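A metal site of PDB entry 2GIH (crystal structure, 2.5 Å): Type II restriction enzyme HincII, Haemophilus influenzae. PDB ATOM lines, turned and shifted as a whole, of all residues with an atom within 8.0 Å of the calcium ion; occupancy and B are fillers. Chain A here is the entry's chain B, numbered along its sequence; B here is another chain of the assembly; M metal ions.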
ATOM      1  N   GLU A  34      -3.726 -15.902 -12.831  1.00  0.00           N
ATOM      2  CA  GLU A  34      -3.317 -16.432 -14.127  1.00  0.00           C
ATOM      3  C   GLU A  34      -2.437 -17.678 -14.112  1.00  0.00           C
ATOM      4  O   GLU A  34      -2.570 -18.546 -14.977  1.00  0.00           O
ATOM      5  CB  GLU A  34      -2.604 -15.330 -14.930  1.00  0.00           C
ATOM      6  N   GLU A  37      -3.724 -21.131 -14.893  1.00  0.00           N
ATOM      7  CA  GLU A  37      -3.862 -21.582 -16.269  1.00  0.00           C
ATOM      8  C   GLU A  37      -2.761 -22.604 -16.513  1.00  0.00           C
ATOM      9  O   GLU A  37      -3.020 -23.701 -17.010  1.00  0.00           O
ATOM     10  CB  GLU A  37      -3.692 -20.381 -17.220  1.00  0.00           C
ATOM     11  CG  GLU A  37      -4.325 -20.515 -18.610  1.00  0.00           C
ATOM     12  CD  GLU A  37      -3.575 -21.434 -19.557  1.00  0.00           C
ATOM     13  OE1 GLU A  37      -3.579 -22.677 -19.338  1.00  0.00           O
ATOM     14  OE2 GLU A  37      -2.983 -20.923 -20.533  1.00  0.00           O
ATOM     15  N   ASP A 110      -3.905 -14.355 -28.487  1.00  0.00           N
ATOM     16  CA  ASP A 110      -4.462 -15.643 -28.907  1.00  0.00           C
ATOM     17  C   ASP A 110      -5.877 -15.937 -28.394  1.00  0.00           C
ATOM     18  O   ASP A 110      -6.210 -15.713 -27.233  1.00  0.00           O
ATOM     19  CB  ASP A 110      -3.519 -16.796 -28.527  1.00  0.00           C
ATOM     20  CG  ASP A 110      -2.236 -16.793 -29.358  1.00  0.00           C
ATOM     21  OD1 ASP A 110      -2.311 -16.835 -30.604  1.00  0.00           O
ATOM     22  OD2 ASP A 110      -1.145 -16.755 -28.751  1.00  0.00           O
ATOM     23  N   THR A 111      -6.707 -16.444 -29.302  1.00  0.00           N
ATOM     24  CA  THR A 111      -8.093 -16.802 -29.010  1.00  0.00           C
ATOM     25  C   THR A 111      -8.263 -17.742 -27.815  1.00  0.00           C
ATOM     26  O   THR A 111      -9.060 -17.489 -26.920  1.00  0.00           O
ATOM     27  CB  THR A 111      -8.755 -17.436 -30.258  1.00  0.00           C
ATOM     28  OG1 THR A 111      -8.814 -16.463 -31.304  1.00  0.00           O
ATOM     29  CG2 THR A 111     -10.177 -17.944 -29.926  1.00  0.00           C
ATOM     30  N   ALA A 112      -7.504 -18.846 -27.810  1.00  0.00           N
ATOM     31  CA  ALA A 112      -7.585 -19.814 -26.725  1.00  0.00           C
ATOM     32  C   ALA A 112      -6.269 -20.005 -25.968  1.00  0.00           C
ATOM     33  O   ALA A 112      -5.192 -19.718 -26.484  1.00  0.00           O
ATOM     34  CB  ALA A 112      -8.033 -21.157 -27.275  1.00  0.00           C
ATOM     35  N   ASP A 113      -6.391 -20.485 -24.732  1.00  0.00           N
ATOM     36  CA  ASP A 113      -5.255 -20.763 -23.883  1.00  0.00           C
ATOM     37  C   ASP A 113      -4.735 -22.166 -24.214  1.00  0.00           C
ATOM     38  O   ASP A 113      -3.560 -22.358 -24.518  1.00  0.00           O
ATOM     39  CB  ASP A 113      -5.679 -20.729 -22.420  1.00  0.00           C
ATOM     40  CG  ASP A 113      -6.073 -19.344 -21.939  1.00  0.00           C
ATOM     41  OD1 ASP A 113      -5.360 -18.367 -22.269  1.00  0.00           O
ATOM     42  OD2 ASP A 113      -7.075 -19.234 -21.208  1.00  0.00           O
ATOM     43  N   ILE A 114      -5.633 -23.133 -24.155  1.00  0.00           N
ATOM     44  CA  ILE A 114      -5.294 -24.506 -24.431  1.00  0.00           C
ATOM     45  C   ILE A 114      -6.151 -24.958 -25.592  1.00  0.00           C
ATOM     46  O   ILE A 114      -7.310 -24.547 -25.718  1.00  0.00           O
ATOM     47  CB  ILE A 114      -5.577 -25.385 -23.213  1.00  0.00           C
ATOM     48  CG1 ILE A 114      -4.876 -24.781 -21.995  1.00  0.00           C
ATOM     49  CG2 ILE A 114      -5.122 -26.822 -23.457  1.00  0.00           C
ATOM     50  CD1 ILE A 114      -5.602 -25.043 -20.710  1.00  0.00           C
ATOM     51  N   LEU A 125     -10.120 -24.287 -25.518  1.00  0.00           N
ATOM     52  CA  LEU A 125     -10.341 -24.104 -24.097  1.00  0.00           C
ATOM     53  C   LEU A 125      -9.745 -22.792 -23.617  1.00  0.00           C
ATOM     54  O   LEU A 125      -8.607 -22.456 -23.950  1.00  0.00           O
ATOM     55  CB  LEU A 125      -9.722 -25.259 -23.298  1.00  0.00           C
ATOM     56  CG  LEU A 125      -9.937 -25.124 -21.787  1.00  0.00           C
ATOM     57  CD1 LEU A 125     -11.410 -25.259 -21.432  1.00  0.00           C
ATOM     58  CD2 LEU A 125      -9.125 -26.188 -21.077  1.00  0.00           C
ATOM     59  N   ASP A 126     -10.544 -22.033 -22.866  1.00  0.00           N
ATOM     60  CA  ASP A 126     -10.100 -20.765 -22.337  1.00  0.00           C
ATOM     61  C   ASP A 126     -10.324 -20.854 -20.836  1.00  0.00           C
ATOM     62  O   ASP A 126     -11.429 -21.120 -20.381  1.00  0.00           O
ATOM     63  CB  ASP A 126     -10.918 -19.618 -22.935  1.00  0.00           C
ATOM     64  CG  ASP A 126     -10.370 -18.244 -22.577  1.00  0.00           C
ATOM     65  OD1 ASP A 126     -10.369 -17.862 -21.392  1.00  0.00           O
ATOM     66  OD2 ASP A 126      -9.922 -17.533 -23.507  1.00  0.00           O
ATOM     67  N   VAL A 127      -9.255 -20.637 -20.067  1.00  0.00           N
ATOM     68  CA  VAL A 127      -9.329 -20.707 -18.615  1.00  0.00           C
ATOM     69  C   VAL A 127      -9.658 -19.347 -18.004  1.00  0.00           C
ATOM     70  O   VAL A 127      -9.033 -18.343 -18.345  1.00  0.00           O
ATOM     71  CB  VAL A 127      -7.982 -21.195 -18.037  1.00  0.00           C
ATOM     72  CG1 VAL A 127      -8.045 -21.277 -16.523  1.00  0.00           C
ATOM     73  CG2 VAL A 127      -7.636 -22.544 -18.641  1.00  0.00           C
ATOM     74  N   LYS A 128     -10.636 -19.329 -17.113  1.00  0.00           N
ATOM     75  CA  LYS A 128     -11.050 -18.109 -16.430  1.00  0.00           C
ATOM     76  C   LYS A 128     -10.709 -18.292 -14.963  1.00  0.00           C
ATOM     77  O   LYS A 128     -10.870 -19.383 -14.413  1.00  0.00           O
ATOM     78  CB  LYS A 128     -12.563 -17.897 -16.578  1.00  0.00           C
ATOM     79  CG  LYS A 128     -13.128 -18.241 -17.941  1.00  0.00           C
ATOM     80  CD  LYS A 128     -12.349 -17.615 -19.095  1.00  0.00           C
ATOM     81  CE  LYS A 128     -12.369 -16.099 -19.045  1.00  0.00           C
ATOM     82  NZ  LYS A 128     -11.681 -15.557 -20.258  1.00  0.00           N
ATOM     83  N   THR A 129     -10.212 -17.232 -14.320  1.00  0.00           N
ATOM     84  CA  THR A 129      -9.872 -17.338 -12.907  1.00  0.00           C
ATOM     85  C   THR A 129     -10.611 -16.254 -12.128  1.00  0.00           C
ATOM     86  O   THR A 129     -10.545 -15.072 -12.464  1.00  0.00           O
ATOM     87  CB  THR A 129      -8.341 -17.227 -12.683  1.00  0.00           C
ATOM     88  OG1 THR A 129      -7.892 -15.916 -13.035  1.00  0.00           O
ATOM     89  CG2 THR A 129      -7.610 -18.246 -13.534  1.00  0.00           C
ATOM     90  N   ASN A 140     -14.375 -10.479 -18.927  1.00  0.00           N
ATOM     91  CA  ASN A 140     -14.431 -10.540 -20.376  1.00  0.00           C
ATOM     92  C   ASN A 140     -14.318 -12.022 -20.716  1.00  0.00           C
ATOM     93  O   ASN A 140     -13.555 -12.758 -20.091  1.00  0.00           O
ATOM     94  CB  ASN A 140     -13.265  -9.776 -21.003  1.00  0.00           C
ATOM     95  CG  ASN A 140     -13.378  -8.267 -20.815  1.00  0.00           C
ATOM     96  OD1 ASN A 140     -14.408  -7.751 -20.374  1.00  0.00           O
ATOM     97  ND2 ASN A 140     -12.316  -7.554 -21.182  1.00  0.00           N
ATOM     98  N   ILE A 141     -15.073 -12.475 -21.711  1.00  0.00           N
ATOM     99  CA  ILE A 141     -15.022 -13.870 -22.110  1.00  0.00           C
ATOM    100  C   ILE A 141     -14.401 -13.969 -23.499  1.00  0.00           C
ATOM    101  O   ILE A 141     -13.442 -14.693 -23.699  1.00  0.00           O
ATOM    102  CB  ILE A 141     -16.429 -14.497 -22.124  1.00  0.00           C
ATOM    103  CG1 ILE A 141     -16.971 -14.542 -20.700  1.00  0.00           C
ATOM    104  CG2 ILE A 141     -16.388 -15.898 -22.746  1.00  0.00           C
ATOM    105  CD1 ILE A 141     -16.091 -15.326 -19.707  1.00  0.00           C
ATOM    106  N   TYR A 167     -15.139 -23.393 -21.556  1.00  0.00           N
ATOM    107  CA  TYR A 167     -14.494 -22.622 -20.515  1.00  0.00           C
ATOM    108  C   TYR A 167     -14.375 -23.377 -19.202  1.00  0.00           C
ATOM    109  O   TYR A 167     -15.174 -24.274 -18.892  1.00  0.00           O
ATOM    110  CB  TYR A 167     -15.286 -21.323 -20.308  1.00  0.00           C
ATOM    111  CG  TYR A 167     -15.298 -20.431 -21.537  1.00  0.00           C
ATOM    112  CD1 TYR A 167     -14.246 -19.552 -21.778  1.00  0.00           C
ATOM    113  CD2 TYR A 167     -16.319 -20.520 -22.486  1.00  0.00           C
ATOM    114  CE1 TYR A 167     -14.198 -18.779 -22.930  1.00  0.00           C
ATOM    115  CE2 TYR A 167     -16.278 -19.736 -23.655  1.00  0.00           C
ATOM    116  CZ  TYR A 167     -15.194 -18.865 -23.864  1.00  0.00           C
ATOM    117  OH  TYR A 167     -15.089 -18.090 -25.007  1.00  0.00           O
ATOM    118  N   LEU A 168     -13.347 -23.012 -18.440  1.00  0.00           N
ATOM    119  CA  LEU A 168     -13.065 -23.608 -17.147  1.00  0.00           C
ATOM    120  C   LEU A 168     -12.772 -22.441 -16.232  1.00  0.00           C
ATOM    121  O   LEU A 168     -11.865 -21.648 -16.497  1.00  0.00           O
ATOM    122  CB  LEU A 168     -11.828 -24.510 -17.257  1.00  0.00           C
ATOM    123  CG  LEU A 168     -11.489 -25.390 -16.047  1.00  0.00           C
ATOM    124  CD1 LEU A 168     -12.604 -26.398 -15.825  1.00  0.00           C
ATOM    125  CD2 LEU A 168     -10.162 -26.104 -16.305  1.00  0.00           C
ATOM    126  P    DC B   7     -10.163 -12.072 -27.661  1.00  0.00           P
ATOM    127  OP1  DC B   7     -10.340 -13.350 -28.401  1.00  0.00           O
ATOM    128  OP2  DC B   7     -11.351 -11.338 -27.168  1.00  0.00           O
ATOM    129  O5'  DC B   7      -9.179 -12.333 -26.440  1.00  0.00           O
ATOM    130  C5'  DC B   7      -7.762 -12.383 -26.663  1.00  0.00           C
ATOM    131  C4'  DC B   7      -6.986 -12.189 -25.371  1.00  0.00           C
ATOM    132  O4'  DC B   7      -6.659 -10.782 -25.193  1.00  0.00           O
ATOM    133  C3'  DC B   7      -7.705 -12.643 -24.102  1.00  0.00           C
ATOM    134  O3'  DC B   7      -7.045 -13.674 -23.398  1.00  0.00           O
ATOM    135  C2'  DC B   7      -7.743 -11.418 -23.205  1.00  0.00           C
ATOM    136  C1'  DC B   7      -6.784 -10.415 -23.821  1.00  0.00           C
ATOM    137  N1   DC B   7      -7.414  -9.081 -23.754  1.00  0.00           N
ATOM    138  C2   DC B   7      -6.766  -8.033 -23.097  1.00  0.00           C
ATOM    139  O2   DC B   7      -5.601  -8.200 -22.700  1.00  0.00           O
ATOM    140  N3   DC B   7      -7.418  -6.857 -22.914  1.00  0.00           N
ATOM    141  C4   DC B   7      -8.666  -6.710 -23.385  1.00  0.00           C
ATOM    142  N4   DC B   7      -9.301  -5.578 -23.131  1.00  0.00           N
ATOM    143  C5   DC B   7      -9.314  -7.747 -24.114  1.00  0.00           C
ATOM    144  C6   DC B   7      -8.658  -8.894 -24.284  1.00  0.00           C
ATOM    145  P    DG B   8      -7.847 -14.442 -22.232  1.00  0.00           P
ATOM    146  OP1  DG B   8      -7.220 -15.780 -22.039  1.00  0.00           O
ATOM    147  OP2  DG B   8      -9.301 -14.360 -22.527  1.00  0.00           O
ATOM    148  O5'  DG B   8      -7.587 -13.543 -20.944  1.00  0.00           O
ATOM    149  C5'  DG B   8      -6.274 -13.065 -20.633  1.00  0.00           C
ATOM    150  C4'  DG B   8      -6.286 -12.317 -19.325  1.00  0.00           C
ATOM    151  O4'  DG B   8      -6.377 -10.880 -19.538  1.00  0.00           O
ATOM    152  C3'  DG B   8      -7.448 -12.703 -18.423  1.00  0.00           C
ATOM    153  O3'  DG B   8      -7.063 -13.180 -17.132  1.00  0.00           O
ATOM    154  C2'  DG B   8      -8.259 -11.433 -18.287  1.00  0.00           C
ATOM    155  C1'  DG B   8      -7.275 -10.316 -18.588  1.00  0.00           C
ATOM    156  N9   DG B   8      -7.961  -9.190 -19.209  1.00  0.00           N
ATOM    157  C8   DG B   8      -8.905  -9.274 -20.201  1.00  0.00           C
ATOM    158  N7   DG B   8      -9.464  -8.126 -20.480  1.00  0.00           N
ATOM    159  C5   DG B   8      -8.837  -7.223 -19.635  1.00  0.00           C
ATOM    160  C6   DG B   8      -9.055  -5.838 -19.460  1.00  0.00           C
ATOM    161  O6   DG B   8      -9.874  -5.112 -20.031  1.00  0.00           O
ATOM    162  N1   DG B   8      -8.212  -5.310 -18.509  1.00  0.00           N
ATOM    163  C2   DG B   8      -7.282  -6.014 -17.804  1.00  0.00           C
ATOM    164  N2   DG B   8      -6.560  -5.288 -16.926  1.00  0.00           N
ATOM    165  N3   DG B   8      -7.075  -7.316 -17.934  1.00  0.00           N
ATOM    166  C4   DG B   8      -7.881  -7.860 -18.866  1.00  0.00           C
ATOM    167  P    DA B   9      -8.122 -14.038 -16.279  1.00  0.00           P
ATOM    168  OP1  DA B   9      -7.543 -14.393 -14.965  1.00  0.00           O
ATOM    169  OP2  DA B   9      -8.654 -15.105 -17.171  1.00  0.00           O
ATOM    170  O5'  DA B   9      -9.305 -12.994 -16.068  1.00  0.00           O
ATOM    171  C5'  DA B   9      -9.874 -12.795 -14.783  1.00  0.00           C
ATOM    172  C4'  DA B   9      -9.348 -11.507 -14.181  1.00  0.00           C
ATOM    173  O4'  DA B   9      -9.413 -10.423 -15.147  1.00  0.00           O
ATOM    174  C3'  DA B   9     -10.201 -11.073 -12.995  1.00  0.00           C
ATOM    175  O3'  DA B   9      -9.363 -10.617 -11.944  1.00  0.00           O
ATOM    176  C2'  DA B   9     -11.075  -9.977 -13.556  1.00  0.00           C
ATOM    177  C1'  DA B   9     -10.223  -9.369 -14.653  1.00  0.00           C
ATOM    178  N9   DA B   9     -11.010  -8.810 -15.764  1.00  0.00           N
ATOM    179  C8   DA B   9     -11.835  -9.475 -16.630  1.00  0.00           C
ATOM    180  N7   DA B   9     -12.453  -8.701 -17.483  1.00  0.00           N
ATOM    181  C5   DA B   9     -12.002  -7.427 -17.170  1.00  0.00           C
ATOM    182  C6   DA B   9     -12.308  -6.155 -17.691  1.00  0.00           C
ATOM    183  N6   DA B   9     -13.176  -5.943 -18.688  1.00  0.00           N
ATOM    184  N1   DA B   9     -11.690  -5.083 -17.148  1.00  0.00           N
ATOM    185  C2   DA B   9     -10.837  -5.282 -16.137  1.00  0.00           C
ATOM    186  N3   DA B   9     -10.476  -6.428 -15.554  1.00  0.00           N
ATOM    187  C4   DA B   9     -11.104  -7.472 -16.119  1.00  0.00           C
HETATM  188 CA    CA M   1      -7.979 -17.385 -20.428  1.00  0.00          CA
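N of Asp 113 is in hydrogen-bond range of O of Leu 125 (3.1 Å). OP2 of DG 8 of chain B is in salt-bridge range of the side-chain amino group of Lys 128, at 3.5 Å. N7 of DG 8 of chain B is in hydrogen-bond range of the side-chain amide nitrogen of Asn 140 (3.0 Å). The backbone NH of Leu 168 sits at hydrogen-bond distance from the backbone carbonyl oxygen of Asp 126, at 3.3 Å. The side-chain carboxylate (OD1) of Asp 126 lies close to the side-chain amino group (NZ) of Lys 128 (2.9 Å).
Within 4 Å of the calcium ion: Asp 113, Asp 126, Val 127 and DG 8 of chain B.
The calcium ion is bound by OD2 of Asp 113 (2.2 Å), OP1 of DG 8 of chain B (2.4 Å), O of Val 127 (2.5 Å) and OD1 of Asp 126 (2.6 Å). The calcium ion has four donor atoms within binding distance.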
